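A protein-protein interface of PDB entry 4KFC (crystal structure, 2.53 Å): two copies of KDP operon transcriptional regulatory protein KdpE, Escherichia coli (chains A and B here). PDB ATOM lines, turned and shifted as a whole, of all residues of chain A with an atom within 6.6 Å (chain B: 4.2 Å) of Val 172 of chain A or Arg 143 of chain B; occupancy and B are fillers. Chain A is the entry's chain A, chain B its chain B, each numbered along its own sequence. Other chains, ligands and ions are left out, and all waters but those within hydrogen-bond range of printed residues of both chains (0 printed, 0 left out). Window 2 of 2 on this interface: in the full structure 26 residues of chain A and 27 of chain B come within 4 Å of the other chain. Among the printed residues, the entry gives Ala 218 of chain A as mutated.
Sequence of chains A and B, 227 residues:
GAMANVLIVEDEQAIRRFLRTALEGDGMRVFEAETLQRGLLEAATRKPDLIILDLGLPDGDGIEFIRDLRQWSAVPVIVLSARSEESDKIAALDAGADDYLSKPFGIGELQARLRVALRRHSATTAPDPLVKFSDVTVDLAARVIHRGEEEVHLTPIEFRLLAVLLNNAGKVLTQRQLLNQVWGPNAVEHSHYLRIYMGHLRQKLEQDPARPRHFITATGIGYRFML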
ATOM      1  N   ASN A 168      17.389  17.559 -18.700  1.00  0.00           N
ATOM      2  CA  ASN A 168      17.192  16.775 -17.481  1.00  0.00           C
ATOM      3  C   ASN A 168      16.069  15.743 -17.605  1.00  0.00           C
ATOM      4  O   ASN A 168      15.306  15.529 -16.663  1.00  0.00           O
ATOM      5  CB  ASN A 168      16.965  17.690 -16.276  1.00  0.00           C
ATOM      6  CG  ASN A 168      18.202  18.487 -15.916  1.00  0.00           C
ATOM      7  OD1 ASN A 168      18.979  18.094 -15.042  1.00  0.00           O
ATOM      8  ND2 ASN A 168      18.399  19.611 -16.600  1.00  0.00           N
ATOM      9  N   GLY A 170      13.490  12.925 -17.556  1.00  0.00           N
ATOM     10  CA  GLY A 170      13.166  11.873 -16.612  1.00  0.00           C
ATOM     11  C   GLY A 170      13.250  12.347 -15.174  1.00  0.00           C
ATOM     12  O   GLY A 170      12.785  11.667 -14.259  1.00  0.00           O
ATOM     13  N   LYS A 171      13.835  13.521 -14.974  1.00  0.00           N
ATOM     14  CA  LYS A 171      14.050  14.049 -13.633  1.00  0.00           C
ATOM     15  C   LYS A 171      13.125  15.233 -13.386  1.00  0.00           C
ATOM     16  O   LYS A 171      12.890  16.036 -14.296  1.00  0.00           O
ATOM     17  CB  LYS A 171      15.514  14.484 -13.479  1.00  0.00           C
ATOM     18  CG  LYS A 171      16.521  13.390 -13.836  1.00  0.00           C
ATOM     19  CD  LYS A 171      17.873  13.957 -14.263  1.00  0.00           C
ATOM     20  CE  LYS A 171      18.633  14.580 -13.106  1.00  0.00           C
ATOM     21  NZ  LYS A 171      19.131  13.566 -12.138  1.00  0.00           N
ATOM     22  N   VAL A 172      12.592  15.350 -12.170  1.00  0.00           N
ATOM     23  CA  VAL A 172      11.842  16.552 -11.823  1.00  0.00           C
ATOM     24  C   VAL A 172      12.772  17.668 -11.358  1.00  0.00           C
ATOM     25  O   VAL A 172      13.648  17.470 -10.514  1.00  0.00           O
ATOM     26  CB  VAL A 172      10.655  16.308 -10.827  1.00  0.00           C
ATOM     27  CG1 VAL A 172      10.420  14.833 -10.601  1.00  0.00           C
ATOM     28  CG2 VAL A 172      10.861  17.041  -9.510  1.00  0.00           C
ATOM     29  N   LEU A 173      12.597  18.834 -11.968  1.00  0.00           N
ATOM     30  CA  LEU A 173      13.332  20.025 -11.606  1.00  0.00           C
ATOM     31  C   LEU A 173      12.423  20.884 -10.753  1.00  0.00           C
ATOM     32  O   LEU A 173      11.217  20.987 -11.017  1.00  0.00           O
ATOM     33  CB  LEU A 173      13.755  20.780 -12.861  1.00  0.00           C
ATOM     34  CG  LEU A 173      14.669  19.973 -13.777  1.00  0.00           C
ATOM     35  CD1 LEU A 173      14.941  20.713 -15.074  1.00  0.00           C
ATOM     36  CD2 LEU A 173      15.970  19.677 -13.049  1.00  0.00           C
ATOM     37  N   THR A 174      12.996  21.485  -9.714  1.00  0.00           N
ATOM     38  CA  THR A 174      12.224  22.327  -8.816  1.00  0.00           C
ATOM     39  C   THR A 174      11.984  23.656  -9.500  1.00  0.00           C
ATOM     40  O   THR A 174      12.678  23.994 -10.465  1.00  0.00           O
ATOM     41  CB  THR A 174      12.944  22.563  -7.478  1.00  0.00           C
ATOM     42  OG1 THR A 174      14.102  23.376  -7.694  1.00  0.00           O
ATOM     43  CG2 THR A 174      13.362  21.242  -6.862  1.00  0.00           C
ATOM     44  N   GLN A 177      15.141  25.977  -9.542  1.00  0.00           N
ATOM     45  CA  GLN A 177      16.208  25.722 -10.503  1.00  0.00           C
ATOM     46  C   GLN A 177      15.791  26.010 -11.943  1.00  0.00           C
ATOM     47  O   GLN A 177      16.603  26.487 -12.737  1.00  0.00           O
ATOM     48  CB  GLN A 177      16.819  24.324 -10.337  1.00  0.00           C
ATOM     49  CG  GLN A 177      15.834  23.180 -10.268  1.00  0.00           C
ATOM     50  CD  GLN A 177      16.489  21.899  -9.782  1.00  0.00           C
ATOM     51  OE1 GLN A 177      15.832  20.871  -9.622  1.00  0.00           O
ATOM     52  NE2 GLN A 177      17.794  21.958  -9.544  1.00  0.00           N
ATOM     53  N   ILE A 216       5.105  16.929 -17.304  1.00  0.00           N
ATOM     54  CA  ILE A 216       4.399  16.545 -16.093  1.00  0.00           C
ATOM     55  C   ILE A 216       4.649  17.513 -14.943  1.00  0.00           C
ATOM     56  O   ILE A 216       5.769  17.982 -14.739  1.00  0.00           O
ATOM     57  CB  ILE A 216       4.807  15.128 -15.659  1.00  0.00           C
ATOM     58  CG1 ILE A 216       4.906  14.211 -16.883  1.00  0.00           C
ATOM     59  CG2 ILE A 216       3.834  14.575 -14.622  1.00  0.00           C
ATOM     60  CD1 ILE A 216       3.605  14.059 -17.659  1.00  0.00           C
ATOM     61  N   ALA A 218       4.899  18.335 -10.974  1.00  0.00           N
ATOM     62  CA  ALA A 218       5.200  17.719  -9.694  1.00  0.00           C
ATOM     63  C   ALA A 218       4.746  18.697  -8.629  1.00  0.00           C
ATOM     64  O   ALA A 218       5.527  19.539  -8.168  1.00  0.00           O
ATOM     65  CB  ALA A 218       6.683  17.436  -9.570  1.00  0.00           C
ATOM     66  N   ILE A 221       6.471  21.022  -6.038  1.00  0.00           N
ATOM     67  CA  ILE A 221       7.898  20.876  -6.302  1.00  0.00           C
ATOM     68  C   ILE A 221       8.334  21.638  -7.553  1.00  0.00           C
ATOM     69  O   ILE A 221       9.085  22.611  -7.467  1.00  0.00           O
ATOM     70  CB  ILE A 221       8.290  19.395  -6.454  1.00  0.00           C
ATOM     71  CG1 ILE A 221       7.869  18.596  -5.215  1.00  0.00           C
ATOM     72  CG2 ILE A 221       9.783  19.269  -6.702  1.00  0.00           C
ATOM     73  CD1 ILE A 221       8.605  19.008  -3.939  1.00  0.00           C
ATOM     74  N   GLY A 222       7.865  21.184  -8.711  1.00  0.00           N
ATOM     75  CA  GLY A 222       8.268  21.765  -9.978  1.00  0.00           C
ATOM     76  C   GLY A 222       7.689  21.036 -11.184  1.00  0.00           C
ATOM     77  O   GLY A 222       6.498  20.721 -11.211  1.00  0.00           O
ATOM     78  N   TYR A 223       8.521  20.777 -12.192  1.00  0.00           N
ATOM     79  CA  TYR A 223       8.037  20.127 -13.416  1.00  0.00           C
ATOM     80  C   TYR A 223       9.033  19.094 -13.907  1.00  0.00           C
ATOM     81  O   TYR A 223      10.137  19.013 -13.392  1.00  0.00           O
ATOM     82  CB  TYR A 223       7.777  21.161 -14.516  1.00  0.00           C
ATOM     83  CG  TYR A 223       6.667  22.122 -14.182  1.00  0.00           C
ATOM     84  CD1 TYR A 223       6.916  23.262 -13.439  1.00  0.00           C
ATOM     85  CD2 TYR A 223       5.370  21.881 -14.600  1.00  0.00           C
ATOM     86  CE1 TYR A 223       5.903  24.140 -13.124  1.00  0.00           C
ATOM     87  CE2 TYR A 223       4.350  22.754 -14.290  1.00  0.00           C
ATOM     88  CZ  TYR A 223       4.624  23.881 -13.553  1.00  0.00           C
ATOM     89  OH  TYR A 223       3.616  24.760 -13.234  1.00  0.00           O
ATOM     90  N   ARG A 224       8.654  18.320 -14.917  1.00  0.00           N
ATOM     91  CA  ARG A 224       9.504  17.236 -15.387  1.00  0.00           C
ATOM     92  C   ARG A 224       9.134  16.802 -16.795  1.00  0.00           C
ATOM     93  O   ARG A 224       7.959  16.680 -17.112  1.00  0.00           O
ATOM     94  CB  ARG A 224       9.389  16.059 -14.416  1.00  0.00           C
ATOM     95  CG  ARG A 224       9.557  14.680 -15.027  1.00  0.00           C
ATOM     96  CD  ARG A 224       9.737  13.642 -13.932  1.00  0.00           C
ATOM     97  NE  ARG A 224       9.200  12.341 -14.306  1.00  0.00           N
ATOM     98  CZ  ARG A 224       8.043  11.861 -13.862  1.00  0.00           C
ATOM     99  NH1 ARG A 224       7.307  12.573 -13.019  1.00  0.00           N
ATOM    100  NH2 ARG A 224       7.630  10.666 -14.255  1.00  0.00           N
ATOM    101  N   PHE A 225      10.134  16.570 -17.639  1.00  0.00           N
ATOM    102  CA  PHE A 225       9.883  16.028 -18.969  1.00  0.00           C
ATOM    103  C   PHE A 225      10.116  14.519 -19.003  1.00  0.00           C
ATOM    104  O   PHE A 225      11.182  14.048 -18.608  1.00  0.00           O
ATOM    105  CB  PHE A 225      10.777  16.707 -20.001  1.00  0.00           C
ATOM    106  CG  PHE A 225      10.791  16.015 -21.332  1.00  0.00           C
ATOM    107  CD1 PHE A 225       9.757  16.207 -22.239  1.00  0.00           C
ATOM    108  CD2 PHE A 225      11.838  15.174 -21.684  1.00  0.00           C
ATOM    109  CE1 PHE A 225       9.768  15.569 -23.475  1.00  0.00           C
ATOM    110  CE2 PHE A 225      11.851  14.532 -22.917  1.00  0.00           C
ATOM    111  CZ  PHE A 225      10.815  14.730 -23.811  1.00  0.00           C
ATOM    112  N   ASP B 139      14.607   6.698  -7.153  1.00  0.00           N
ATOM    113  CA  ASP B 139      15.625   7.567  -7.747  1.00  0.00           C
ATOM    114  C   ASP B 139      15.553   8.919  -7.033  1.00  0.00           C
ATOM    115  O   ASP B 139      14.720   9.769  -7.374  1.00  0.00           O
ATOM    116  CB  ASP B 139      15.381   7.728  -9.252  1.00  0.00           C
ATOM    117  CG  ASP B 139      16.513   8.463  -9.966  1.00  0.00           C
ATOM    118  OD1 ASP B 139      17.258   9.229  -9.315  1.00  0.00           O
ATOM    119  OD2 ASP B 139      16.635   8.300 -11.199  1.00  0.00           O
ATOM    120  N   LEU B 140      16.416   9.106  -6.037  1.00  0.00           N
ATOM    121  CA  LEU B 140      16.351  10.276  -5.171  1.00  0.00           C
ATOM    122  C   LEU B 140      16.565  11.589  -5.919  1.00  0.00           C
ATOM    123  O   LEU B 140      15.797  12.534  -5.743  1.00  0.00           O
ATOM    124  CB  LEU B 140      17.342  10.131  -4.014  1.00  0.00           C
ATOM    125  CG  LEU B 140      16.922   9.133  -2.933  1.00  0.00           C
ATOM    126  CD1 LEU B 140      17.985   8.996  -1.849  1.00  0.00           C
ATOM    127  CD2 LEU B 140      15.589   9.554  -2.328  1.00  0.00           C
ATOM    128  N   ALA B 141      17.598  11.637  -6.756  1.00  0.00           N
ATOM    129  CA  ALA B 141      17.909  12.835  -7.530  1.00  0.00           C
ATOM    130  C   ALA B 141      16.768  13.197  -8.472  1.00  0.00           C
ATOM    131  O   ALA B 141      16.424  14.369  -8.624  1.00  0.00           O
ATOM    132  CB  ALA B 141      19.193  12.636  -8.312  1.00  0.00           C
ATOM    133  N   ALA B 142      16.184  12.183  -9.100  1.00  0.00           N
ATOM    134  CA  ALA B 142      15.107  12.401 -10.057  1.00  0.00           C
ATOM    135  C   ALA B 142      13.740  12.558  -9.399  1.00  0.00           C
ATOM    136  O   ALA B 142      12.774  12.907 -10.079  1.00  0.00           O
ATOM    137  CB  ALA B 142      15.068  11.278 -11.080  1.00  0.00           C
ATOM    138  N   ARG B 143      13.659  12.296  -8.093  1.00  0.00           N
ATOM    139  CA  ARG B 143      12.378  12.319  -7.376  1.00  0.00           C
ATOM    140  C   ARG B 143      11.318  11.449  -8.048  1.00  0.00           C
ATOM    141  O   ARG B 143      10.155  11.842  -8.133  1.00  0.00           O
ATOM    142  CB  ARG B 143      11.841  13.751  -7.234  1.00  0.00           C
ATOM    143  CG  ARG B 143      12.735  14.687  -6.426  1.00  0.00           C
ATOM    144  CD  ARG B 143      12.033  16.015  -6.166  1.00  0.00           C
ATOM    145  NE  ARG B 143      10.808  15.834  -5.389  1.00  0.00           N
ATOM    146  CZ  ARG B 143      10.706  16.069  -4.084  1.00  0.00           C
ATOM    147  NH1 ARG B 143      11.755  16.516  -3.403  1.00  0.00           N
ATOM    148  NH2 ARG B 143       9.552  15.869  -3.463  1.00  0.00           N
ATOM    149  N   VAL B 144      11.719  10.275  -8.529  1.00  0.00           N
ATOM    150  CA  VAL B 144      10.780   9.356  -9.166  1.00  0.00           C
ATOM    151  C   VAL B 144      10.812   7.972  -8.513  1.00  0.00           C
ATOM    152  O   VAL B 144      11.876   7.364  -8.371  1.00  0.00           O
ATOM    153  CB  VAL B 144      11.038   9.251 -10.679  1.00  0.00           C
ATOM    154  CG1 VAL B 144      10.221   8.125 -11.289  1.00  0.00           C
ATOM    155  CG2 VAL B 144      10.703  10.571 -11.353  1.00  0.00           C
ATOM    156  N   PRO B 156       5.103  15.708  -1.629  1.00  0.00           N
ATOM    157  CA  PRO B 156       6.386  16.235  -1.140  1.00  0.00           C
ATOM    158  C   PRO B 156       6.799  15.737   0.245  1.00  0.00           C
ATOM    159  O   PRO B 156       7.964  15.367   0.439  1.00  0.00           O
ATOM    160  CB  PRO B 156       6.141  17.743  -1.098  1.00  0.00           C
ATOM    161  CG  PRO B 156       5.179  17.976  -2.215  1.00  0.00           C
ATOM    162  CD  PRO B 156       4.274  16.769  -2.237  1.00  0.00           C
ATOM    163  N   PHE B 159       7.710  12.122   0.255  1.00  0.00           N
ATOM    164  CA  PHE B 159       9.031  11.931  -0.332  1.00  0.00           C
ATOM    165  C   PHE B 159      10.147  12.322   0.633  1.00  0.00           C
ATOM    166  O   PHE B 159      11.150  11.619   0.727  1.00  0.00           O
ATOM    167  CB  PHE B 159       9.175  12.698  -1.652  1.00  0.00           C
ATOM    168  CG  PHE B 159      10.465  12.422  -2.370  1.00  0.00           C
ATOM    169  CD1 PHE B 159      10.585  11.323  -3.207  1.00  0.00           C
ATOM    170  CD2 PHE B 159      11.567  13.252  -2.199  1.00  0.00           C
ATOM    171  CE1 PHE B 159      11.779  11.057  -3.869  1.00  0.00           C
ATOM    172  CE2 PHE B 159      12.765  12.992  -2.859  1.00  0.00           C
ATOM    173  CZ  PHE B 159      12.868  11.893  -3.694  1.00  0.00           C
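The backbone carbonyl oxygen of Ala 142 of chain B lies close to the backbone NH of Val 172 of chain A, 3.2 Å away.
Printed residues of chain A that touch a printed residue of chain B: Gly 170, Lys 171, Val 172, Ile 221 and Arg 224.
Among the printed residues, no Asp or Glu carboxylate lies within 4 Å of a Lys or Arg side-chain nitrogen of the other chain.
No position is printed for both chains.
Of the 9 pairs that touch across the chains among the printed residues, none has its exchanged pair printed and touching as well.
The side-chain carboxylate (OD1) of Asp 139 of chain B is in hydrogen-bond range of the backbone NH (N) of Ala 142 of chain B, 3.2 Å away.
The backbone NH (N) of Gly 170 of chain A is in hydrogen-bond range of the backbone carbonyl oxygen (O) of Phe 225 of chain A, 2.8 Å away.
The backbone NH (N) of Asp 139 of chain B is in hydrogen-bond range of the backbone carbonyl oxygen (O) of Val 144 of chain B (3.1 Å).
N of Ile 216 of chain A sits at hydrogen-bond distance from O of Arg 224 of chain A (2.9 Å).
Among the printed residues, pairs that only touch across the chains: Gly 170 of chain A with Ala 142 of chain B, Gly 170 of chain A with Val 144 of chain B, Lys 171 of chain A with Ala 141 of chain B, Lys 171 of chain A with Ala 142 of chain B, Val 172 of chain A with Arg 143 of chain B, Ile 221 of chain A with Arg 143 of chain B, Ile 221 of chain A with Pro 156 of chain B and Arg 224 of chain A with Val 144 of chain B.
Of chain B, only Ala 142 (3.1 Å) and Arg 143 (3.7 Å) come within 4 Å of Val 172 of chain A.
Arg 143 of chain B touches just these residues of chain A: Val 172 and Ile 221.
Printed residues of chain A within 4 Å of Pro 156 of chain B: Ile 221 (3.97 Å).
Of the printed residues of chain A, Ala 141 of chain B touches Lys 171.
Tyr 223 of chain A touches none of the printed residues of chain B.
Gly 222 of chain A touches none of the printed residues of chain B.
The nearest residue of chain A that does not touch Arg 143 of chain B is Thr 174 of chain A (5.4 Å).
The nearest printed residue of chain B that does not touch Ile 221 of chain A is Phe 159 of chain B (6.7 Å).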
